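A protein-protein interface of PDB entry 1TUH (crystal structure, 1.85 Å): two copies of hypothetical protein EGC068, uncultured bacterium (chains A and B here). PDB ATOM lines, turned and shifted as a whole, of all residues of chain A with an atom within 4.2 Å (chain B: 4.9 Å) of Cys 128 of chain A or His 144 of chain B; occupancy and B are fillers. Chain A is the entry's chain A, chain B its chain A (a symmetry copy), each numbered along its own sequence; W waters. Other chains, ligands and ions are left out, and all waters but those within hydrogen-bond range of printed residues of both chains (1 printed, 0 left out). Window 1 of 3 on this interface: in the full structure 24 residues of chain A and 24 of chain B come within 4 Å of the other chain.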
ATOM      1  N   ILE A 109      34.739  12.045  11.906  1.00  0.00           N
ATOM      2  CA  ILE A 109      33.812  11.489  12.903  1.00  0.00           C
ATOM      3  C   ILE A 109      34.005  12.190  14.242  1.00  0.00           C
ATOM      4  O   ILE A 109      35.145  12.392  14.718  1.00  0.00           O
ATOM      5  CB  ILE A 109      34.002   9.979  13.042  1.00  0.00           C
ATOM      6  CG1 ILE A 109      33.427   9.297  11.814  1.00  0.00           C
ATOM      7  CG2 ILE A 109      33.360   9.401  14.325  1.00  0.00           C
ATOM      8  CD1 ILE A 109      33.799   7.781  11.701  1.00  0.00           C
ATOM      9  N   GLY A 110      32.869  12.485  14.849  1.00  0.00           N
ATOM     10  CA  GLY A 110      32.812  12.877  16.256  1.00  0.00           C
ATOM     11  C   GLY A 110      32.345  11.643  17.046  1.00  0.00           C
ATOM     12  O   GLY A 110      31.352  11.031  16.691  1.00  0.00           O
ATOM     13  N   ILE A 111      33.125  11.227  18.042  1.00  0.00           N
ATOM     14  CA  ILE A 111      32.665  10.244  19.070  1.00  0.00           C
ATOM     15  C   ILE A 111      32.241  11.046  20.263  1.00  0.00           C
ATOM     16  O   ILE A 111      33.039  11.815  20.836  1.00  0.00           O
ATOM     17  CB  ILE A 111      33.779   9.259  19.504  1.00  0.00           C
ATOM     18  CG1 ILE A 111      34.477   8.605  18.311  1.00  0.00           C
ATOM     19  CG2 ILE A 111      33.225   8.200  20.467  1.00  0.00           C
ATOM     20  CD1 ILE A 111      35.571   7.607  18.661  1.00  0.00           C
ATOM     21  N   CYS A 127      27.769   7.543  20.847  1.00  0.00           N
ATOM     22  CA  CYS A 127      27.439   7.720  19.428  1.00  0.00           C
ATOM     23  C   CYS A 127      28.696   8.082  18.630  1.00  0.00           C
ATOM     24  O   CYS A 127      29.562   8.769  19.171  1.00  0.00           O
ATOM     25  CB  CYS A 127      26.398   8.854  19.319  1.00  0.00           C
ATOM     26  SG  CYS A 127      25.802   9.149  17.630  1.00  0.00           S
ATOM     27  N   CYS A 128      28.808   7.571  17.402  1.00  0.00           N
ATOM     28  CA  CYS A 128      29.729   8.134  16.372  1.00  0.00           C
ATOM     29  C   CYS A 128      28.914   8.798  15.271  1.00  0.00           C
ATOM     30  O   CYS A 128      28.047   8.149  14.651  1.00  0.00           O
ATOM     31  CB  CYS A 128      30.552   7.051  15.758  1.00  0.00           C
ATOM     32  SG  CYS A 128      31.625   6.125  16.887  1.00  0.00           S
ATOM     33  N   ILE A 129      29.157  10.101  15.062  1.00  0.00           N
ATOM     34  CA  ILE A 129      28.572  10.774  13.909  1.00  0.00           C
ATOM     35  C   ILE A 129      29.561  10.854  12.817  1.00  0.00           C
ATOM     36  O   ILE A 129      30.672  11.359  13.042  1.00  0.00           O
ATOM     37  CB  ILE A 129      28.067  12.176  14.238  1.00  0.00           C
ATOM     38  CG1 ILE A 129      27.004  12.158  15.342  1.00  0.00           C
ATOM     39  CG2 ILE A 129      27.508  12.831  12.995  1.00  0.00           C
ATOM     40  CD1 ILE A 129      26.664  13.568  15.808  1.00  0.00           C
ATOM     41  N   VAL A 130      29.188  10.346  11.641  1.00  0.00           N
ATOM     42  CA  VAL A 130      30.005  10.523  10.407  1.00  0.00           C
ATOM     43  C   VAL A 130      29.554  11.804   9.721  1.00  0.00           C
ATOM     44  O   VAL A 130      28.417  11.946   9.405  1.00  0.00           O
ATOM     45  CB  VAL A 130      29.866   9.324   9.452  1.00  0.00           C
ATOM     46  CG1 VAL A 130      30.644   9.546   8.178  1.00  0.00           C
ATOM     47  CG2 VAL A 130      30.253   8.004  10.189  1.00  0.00           C
ATOM     48  N   ARG A 142      25.543  11.475  10.014  1.00  0.00           N
ATOM     49  CA  ARG A 142      24.901  10.183  10.253  1.00  0.00           C
ATOM     50  C   ARG A 142      25.258   9.686  11.602  1.00  0.00           C
ATOM     51  O   ARG A 142      26.411   9.336  11.835  1.00  0.00           O
ATOM     52  CB  ARG A 142      25.328   9.183   9.200  1.00  0.00           C
ATOM     53  CG  ARG A 142      24.571   7.835   9.315  1.00  0.00           C
ATOM     54  CD  ARG A 142      24.934   6.809   8.232  1.00  0.00           C
ATOM     55  NE  ARG A 142      24.408   7.232   6.952  1.00  0.00           N
ATOM     56  CZ  ARG A 142      23.177   6.932   6.490  1.00  0.00           C
ATOM     57  NH1 ARG A 142      22.352   6.176   7.184  1.00  0.00           N
ATOM     58  NH2 ARG A 142      22.791   7.411   5.316  1.00  0.00           N
ATOM     59  N   GLU A 143      24.260   9.662  12.480  1.00  0.00           N
ATOM     60  CA  GLU A 143      24.386   9.136  13.856  1.00  0.00           C
ATOM     61  C   GLU A 143      24.471   7.599  13.865  1.00  0.00           C
ATOM     62  O   GLU A 143      23.550   6.907  13.318  1.00  0.00           O
ATOM     63  CB  GLU A 143      23.154   9.580  14.647  1.00  0.00           C
ATOM     64  CG  GLU A 143      23.102  11.055  15.054  1.00  0.00           C
ATOM     65  CD  GLU A 143      21.703  11.577  15.380  1.00  0.00           C
ATOM     66  OE1 GLU A 143      20.728  10.951  15.000  1.00  0.00           O
ATOM     67  OE2 GLU A 143      21.593  12.659  15.960  1.00  0.00           O
ATOM     68  N   HIS A 144      25.464   7.058  14.591  1.00  0.00           N
ATOM     69  CA  HIS A 144      25.565   5.662  14.839  1.00  0.00           C
ATOM     70  C   HIS A 144      25.639   5.465  16.373  1.00  0.00           C
ATOM     71  O   HIS A 144      26.708   5.596  16.976  1.00  0.00           O
ATOM     72  CB  HIS A 144      26.842   5.019  14.253  1.00  0.00           C
ATOM     73  CG  HIS A 144      26.998   5.155  12.769  1.00  0.00           C
ATOM     74  ND1 HIS A 144      27.196   6.364  12.147  1.00  0.00           N
ATOM     75  CD2 HIS A 144      27.016   4.217  11.797  1.00  0.00           C
ATOM     76  CE1 HIS A 144      27.302   6.165  10.842  1.00  0.00           C
ATOM     77  NE2 HIS A 144      27.200   4.866  10.605  1.00  0.00           N
ATOM     78  N   TYR A 146      25.632   3.284  19.827  1.00  0.00           N
ATOM     79  CA  TYR A 146      26.041   1.962  20.199  1.00  0.00           C
ATOM     80  C   TYR A 146      24.776   1.242  20.663  1.00  0.00           C
ATOM     81  O   TYR A 146      24.319   0.380  19.992  1.00  0.00           O
ATOM     82  CB  TYR A 146      27.108   1.997  21.321  1.00  0.00           C
ATOM     83  CG  TYR A 146      27.593   0.601  21.717  1.00  0.00           C
ATOM     84  CD1 TYR A 146      28.474  -0.120  20.927  1.00  0.00           C
ATOM     85  CD2 TYR A 146      27.127  -0.011  22.897  1.00  0.00           C
ATOM     86  CE1 TYR A 146      28.877  -1.373  21.267  1.00  0.00           C
ATOM     87  CE2 TYR A 146      27.534  -1.278  23.267  1.00  0.00           C
ATOM     88  CZ  TYR A 146      28.412  -1.962  22.469  1.00  0.00           C
ATOM     89  OH  TYR A 146      28.846  -3.212  22.795  1.00  0.00           O
ATOM     90  N   ILE B 109      38.960   4.638  13.265  1.00  0.00           N
ATOM     91  CA  ILE B 109      37.658   4.044  12.926  1.00  0.00           C
ATOM     92  C   ILE B 109      37.701   3.465  11.517  1.00  0.00           C
ATOM     93  O   ILE B 109      38.193   4.105  10.560  1.00  0.00           O
ATOM     94  CB  ILE B 109      36.537   5.074  13.062  1.00  0.00           C
ATOM     95  CG1 ILE B 109      36.278   5.326  14.536  1.00  0.00           C
ATOM     96  CG2 ILE B 109      35.230   4.647  12.353  1.00  0.00           C
ATOM     97  CD1 ILE B 109      35.350   6.555  14.813  1.00  0.00           C
ATOM     98  N   GLY B 126      25.295  -0.992   7.873  1.00  0.00           N
ATOM     99  CA  GLY B 126      26.499  -0.145   7.921  1.00  0.00           C
ATOM    100  C   GLY B 126      26.988  -0.147   9.354  1.00  0.00           C
ATOM    101  O   GLY B 126      26.204  -0.234  10.307  1.00  0.00           O
ATOM    102  N   CYS B 127      28.296   0.046   9.527  1.00  0.00           N
ATOM    103  CA  CYS B 127      28.892   0.006  10.868  1.00  0.00           C
ATOM    104  C   CYS B 127      30.117   0.924  10.933  1.00  0.00           C
ATOM    105  O   CYS B 127      30.819   1.045   9.930  1.00  0.00           O
ATOM    106  CB  CYS B 127      29.306  -1.451  11.162  1.00  0.00           C
ATOM    107  SG  CYS B 127      29.983  -1.705  12.827  1.00  0.00           S
ATOM    108  N   CYS B 128      30.317   1.595  12.070  1.00  0.00           N
ATOM    109  CA  CYS B 128      31.635   2.187  12.439  1.00  0.00           C
ATOM    110  C   CYS B 128      32.232   1.411  13.604  1.00  0.00           C
ATOM    111  O   CYS B 128      31.593   1.283  14.668  1.00  0.00           O
ATOM    112  CB  CYS B 128      31.471   3.610  12.859  1.00  0.00           C
ATOM    113  SG  CYS B 128      30.786   4.736  11.615  1.00  0.00           S
ATOM    114  N   ILE B 129      33.433   0.853  13.387  1.00  0.00           N
ATOM    115  CA  ILE B 129      34.169   0.257  14.495  1.00  0.00           C
ATOM    116  C   ILE B 129      35.178   1.208  14.998  1.00  0.00           C
ATOM    117  O   ILE B 129      35.997   1.698  14.203  1.00  0.00           O
ATOM    118  CB  ILE B 129      34.853  -1.052  14.114  1.00  0.00           C
ATOM    119  CG1 ILE B 129      33.850  -2.101  13.619  1.00  0.00           C
ATOM    120  CG2 ILE B 129      35.627  -1.596  15.294  1.00  0.00           C
ATOM    121  CD1 ILE B 129      34.559  -3.319  13.045  1.00  0.00           C
ATOM    122  N   VAL B 130      35.126   1.497  16.299  1.00  0.00           N
ATOM    123  CA  VAL B 130      36.190   2.290  16.979  1.00  0.00           C
ATOM    124  C   VAL B 130      37.250   1.324  17.485  1.00  0.00           C
ATOM    125  O   VAL B 130      36.953   0.441  18.224  1.00  0.00           O
ATOM    126  CB  VAL B 130      35.626   3.126  18.141  1.00  0.00           C
ATOM    127  CG1 VAL B 130      36.723   3.871  18.862  1.00  0.00           C
ATOM    128  CG2 VAL B 130      34.483   4.057  17.627  1.00  0.00           C
ATOM    129  N   ARG B 142      34.953  -1.601  19.053  1.00  0.00           N
ATOM    130  CA  ARG B 142      33.557  -1.360  19.415  1.00  0.00           C
ATOM    131  C   ARG B 142      32.761  -1.090  18.196  1.00  0.00           C
ATOM    132  O   ARG B 142      32.944  -0.051  17.569  1.00  0.00           O
ATOM    133  CB  ARG B 142      33.459  -0.191  20.372  1.00  0.00           C
ATOM    134  CG  ARG B 142      32.019   0.024  20.905  1.00  0.00           C
ATOM    135  CD  ARG B 142      31.883   1.167  21.920  1.00  0.00           C
ATOM    136  NE  ARG B 142      32.512   0.797  23.171  1.00  0.00           N
ATOM    137  CZ  ARG B 142      31.896   0.145  24.177  1.00  0.00           C
ATOM    138  NH1 ARG B 142      30.622  -0.182  24.102  1.00  0.00           N
ATOM    139  NH2 ARG B 142      32.589  -0.176  25.260  1.00  0.00           N
ATOM    140  N   GLU B 143      31.883  -2.034  17.872  1.00  0.00           N
ATOM    141  CA  GLU B 143      30.942  -1.928  16.736  1.00  0.00           C
ATOM    142  C   GLU B 143      29.807  -0.932  17.036  1.00  0.00           C
ATOM    143  O   GLU B 143      29.077  -1.091  18.070  1.00  0.00           O
ATOM    144  CB  GLU B 143      30.346  -3.314  16.484  1.00  0.00           C
ATOM    145  CG  GLU B 143      31.269  -4.340  15.820  1.00  0.00           C
ATOM    146  CD  GLU B 143      30.855  -5.798  16.029  1.00  0.00           C
ATOM    147  OE1 GLU B 143      30.078  -6.075  16.926  1.00  0.00           O
ATOM    148  OE2 GLU B 143      31.375  -6.668  15.328  1.00  0.00           O
ATOM    149  N   HIS B 144      29.553  -0.010  16.093  1.00  0.00           N
ATOM    150  CA  HIS B 144      28.428   0.857  16.146  1.00  0.00           C
ATOM    151  C   HIS B 144      27.645   0.689  14.822  1.00  0.00           C
ATOM    152  O   HIS B 144      27.993   1.288  13.801  1.00  0.00           O
ATOM    153  CB  HIS B 144      28.805   2.353  16.245  1.00  0.00           C
ATOM    154  CG  HIS B 144      29.630   2.724  17.439  1.00  0.00           C
ATOM    155  ND1 HIS B 144      30.918   2.281  17.623  1.00  0.00           N
ATOM    156  CD2 HIS B 144      29.347   3.526  18.489  1.00  0.00           C
ATOM    157  CE1 HIS B 144      31.385   2.776  18.759  1.00  0.00           C
ATOM    158  NE2 HIS B 144      30.450   3.540  19.302  1.00  0.00           N
ATOM    159  N   PHE B 145      26.606  -0.125  14.823  1.00  0.00           N
ATOM    160  CA  PHE B 145      25.769  -0.318  13.642  1.00  0.00           C
ATOM    161  C   PHE B 145      24.793   0.837  13.524  1.00  0.00           C
ATOM    162  O   PHE B 145      24.423   1.472  14.516  1.00  0.00           O
ATOM    163  CB  PHE B 145      24.991  -1.635  13.724  1.00  0.00           C
ATOM    164  CG  PHE B 145      25.845  -2.804  13.766  1.00  0.00           C
ATOM    165  CD1 PHE B 145      26.363  -3.305  12.585  1.00  0.00           C
ATOM    166  CD2 PHE B 145      26.203  -3.380  14.979  1.00  0.00           C
ATOM    167  CE1 PHE B 145      27.224  -4.410  12.565  1.00  0.00           C
ATOM    168  CE2 PHE B 145      27.066  -4.449  14.980  1.00  0.00           C
ATOM    169  CZ  PHE B 145      27.566  -4.981  13.760  1.00  0.00           C
ATOM    170  N   TYR B 146      24.472   1.230  12.306  1.00  0.00           N
ATOM    171  CA  TYR B 146      23.498   2.260  12.101  1.00  0.00           C
ATOM    172  C   TYR B 146      22.142   1.628  12.410  1.00  0.00           C
ATOM    173  O   TYR B 146      21.559   1.954  13.388  1.00  0.00           O
ATOM    174  CB  TYR B 146      23.546   2.801  10.650  1.00  0.00           C
ATOM    175  CG  TYR B 146      22.540   3.928  10.407  1.00  0.00           C
ATOM    176  CD1 TYR B 146      22.757   5.214  10.874  1.00  0.00           C
ATOM    177  CD2 TYR B 146      21.336   3.679   9.720  1.00  0.00           C
ATOM    178  CE1 TYR B 146      21.846   6.206  10.683  1.00  0.00           C
ATOM    179  CE2 TYR B 146      20.403   4.674   9.505  1.00  0.00           C
ATOM    180  CZ  TYR B 146      20.650   5.938   9.971  1.00  0.00           C
ATOM    181  OH  TYR B 146      19.762   6.955   9.779  1.00  0.00           O
HETATM  182  O   HOH W   1      24.817  -0.254  17.165  1.00  0.00           O
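A ring nitrogen (NE2) of His 144 of chain B sits at hydrogen-bond distance from the side-chain sulfur (SG) of Cys 128 of chain A (3.7 Å). The side-chain sulfur (SG) of Cys 128 of chain B is in hydrogen-bond range of a ring nitrogen (NE2) of His 144 of chain A, 3.7 Å away.
N of His 144 of chain A is in hydrogen-bond range of SG of Cys 127 of chain A. The backbone carbonyl oxygen (O) of Cys 128 of chain A lies within hydrogen-bond range of the backbone NH (N) of His 144 of chain A, 2.8 Å away. The backbone NH (N) of Val 130 of chain A lies within hydrogen-bond range of the backbone carbonyl oxygen (O) of Arg 142 of chain A, at 3.0 Å. A ring nitrogen (ND1) of His 144 of chain A is in hydrogen-bond range of the backbone carbonyl oxygen of Arg 142 of chain A (3.1 Å). The backbone carbonyl oxygen of Gly 126 of chain B lies within hydrogen-bond range of the backbone NH of Tyr 146 of chain B, at 3.0 Å. The backbone carbonyl oxygen of Arg 142 of chain B lies within hydrogen-bond range of the backbone NH of Val 130 of chain B (3.0 Å).
Ile 109 of chain B touches Ile 109 of chain A. Ile 111 of chain A touches Ile 109 of chain B (CD1 to CD1, 3.995 Å). Cys 128 of chain A touches Val 130 of chain B. SG of Cys 128 of chain B touches CG2 of Val 130 of chain A (3.6 Å). CZ of Tyr 146 of chain B touches NH1 of Arg 142 of chain A (3.3 Å). Glu 143 of chain A touches Tyr 146 of chain B. His 144 of chain A touches His 144 of chain B. His 144 of chain A touches Tyr 146 of chain B (CD2 to CB, 3.9 Å). CD1 of Tyr 146 of chain A touches O of Glu 143 of chain B, 3.1 Å away. His 144 of chain B touches Tyr 146 of chain A.
Printed residues of chain B within 4 Å of Ile 111 of chain A: Ile 109 (3.995 Å) and Val 130 (3.9 Å). Of chain B, only Val 130 and His 144 come within 4 Å of Cys 128 of chain A. Gly 126 of chain B touches none of the printed residues of chain A. Printed residues of chain A within 4 Å of Glu 143 of chain B: Tyr 146. His 144 of chain B touches three residues of chain A. Of the printed residues of chain A, Tyr 146 of chain B touches Arg 142 (3.3 Å), Glu 143 (3.1 Å) and His 144 (3.9 Å). The nearest printed residue of chain A that does not touch His 144 of chain B is Cys 127 of chain A (4.6 Å).
Printed residues of chain B that touch a printed residue of chain A: Ile 109, Cys 128, Val 130, Arg 142, Glu 143, His 144 and Tyr 146. Of the 11 printed residues of chain A, 8 touch a printed residue of chain B. Printed residues of chain A that touch a printed residue of chain B: Ile 109, Ile 111, Cys 128, Val 130, Arg 142, Glu 143, His 144 and Tyr 146. Hydrophobic or aromatic side chains of chain A within 4 Å of the printed part of chain B: Ile 109, Ile 111, Val 130, His 144 and Tyr 146.
Ile 109 of chain B touches its own counterpart, Ile 109 of chain A. Cys 128 of chain A touches His 144 of chain B, and with the chains exchanged His 144 of chain A touches Cys 128 of chain B. Arg 142 of chain A touches Tyr 146 of chain B, and with the chains exchanged Tyr 146 of chain A touches Arg 142 of chain B. His 144 of chain A touches Tyr 146 of chain B, and with the chains exchanged Tyr 146 of chain A touches His 144 of chain B. 9 positions are printed for both chains.
Water W1 bridges the backbone carbonyl oxygen of Tyr 146 of chain A (2.9 Å) and the backbone NH of Phe 145 of chain B (2.9 Å).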
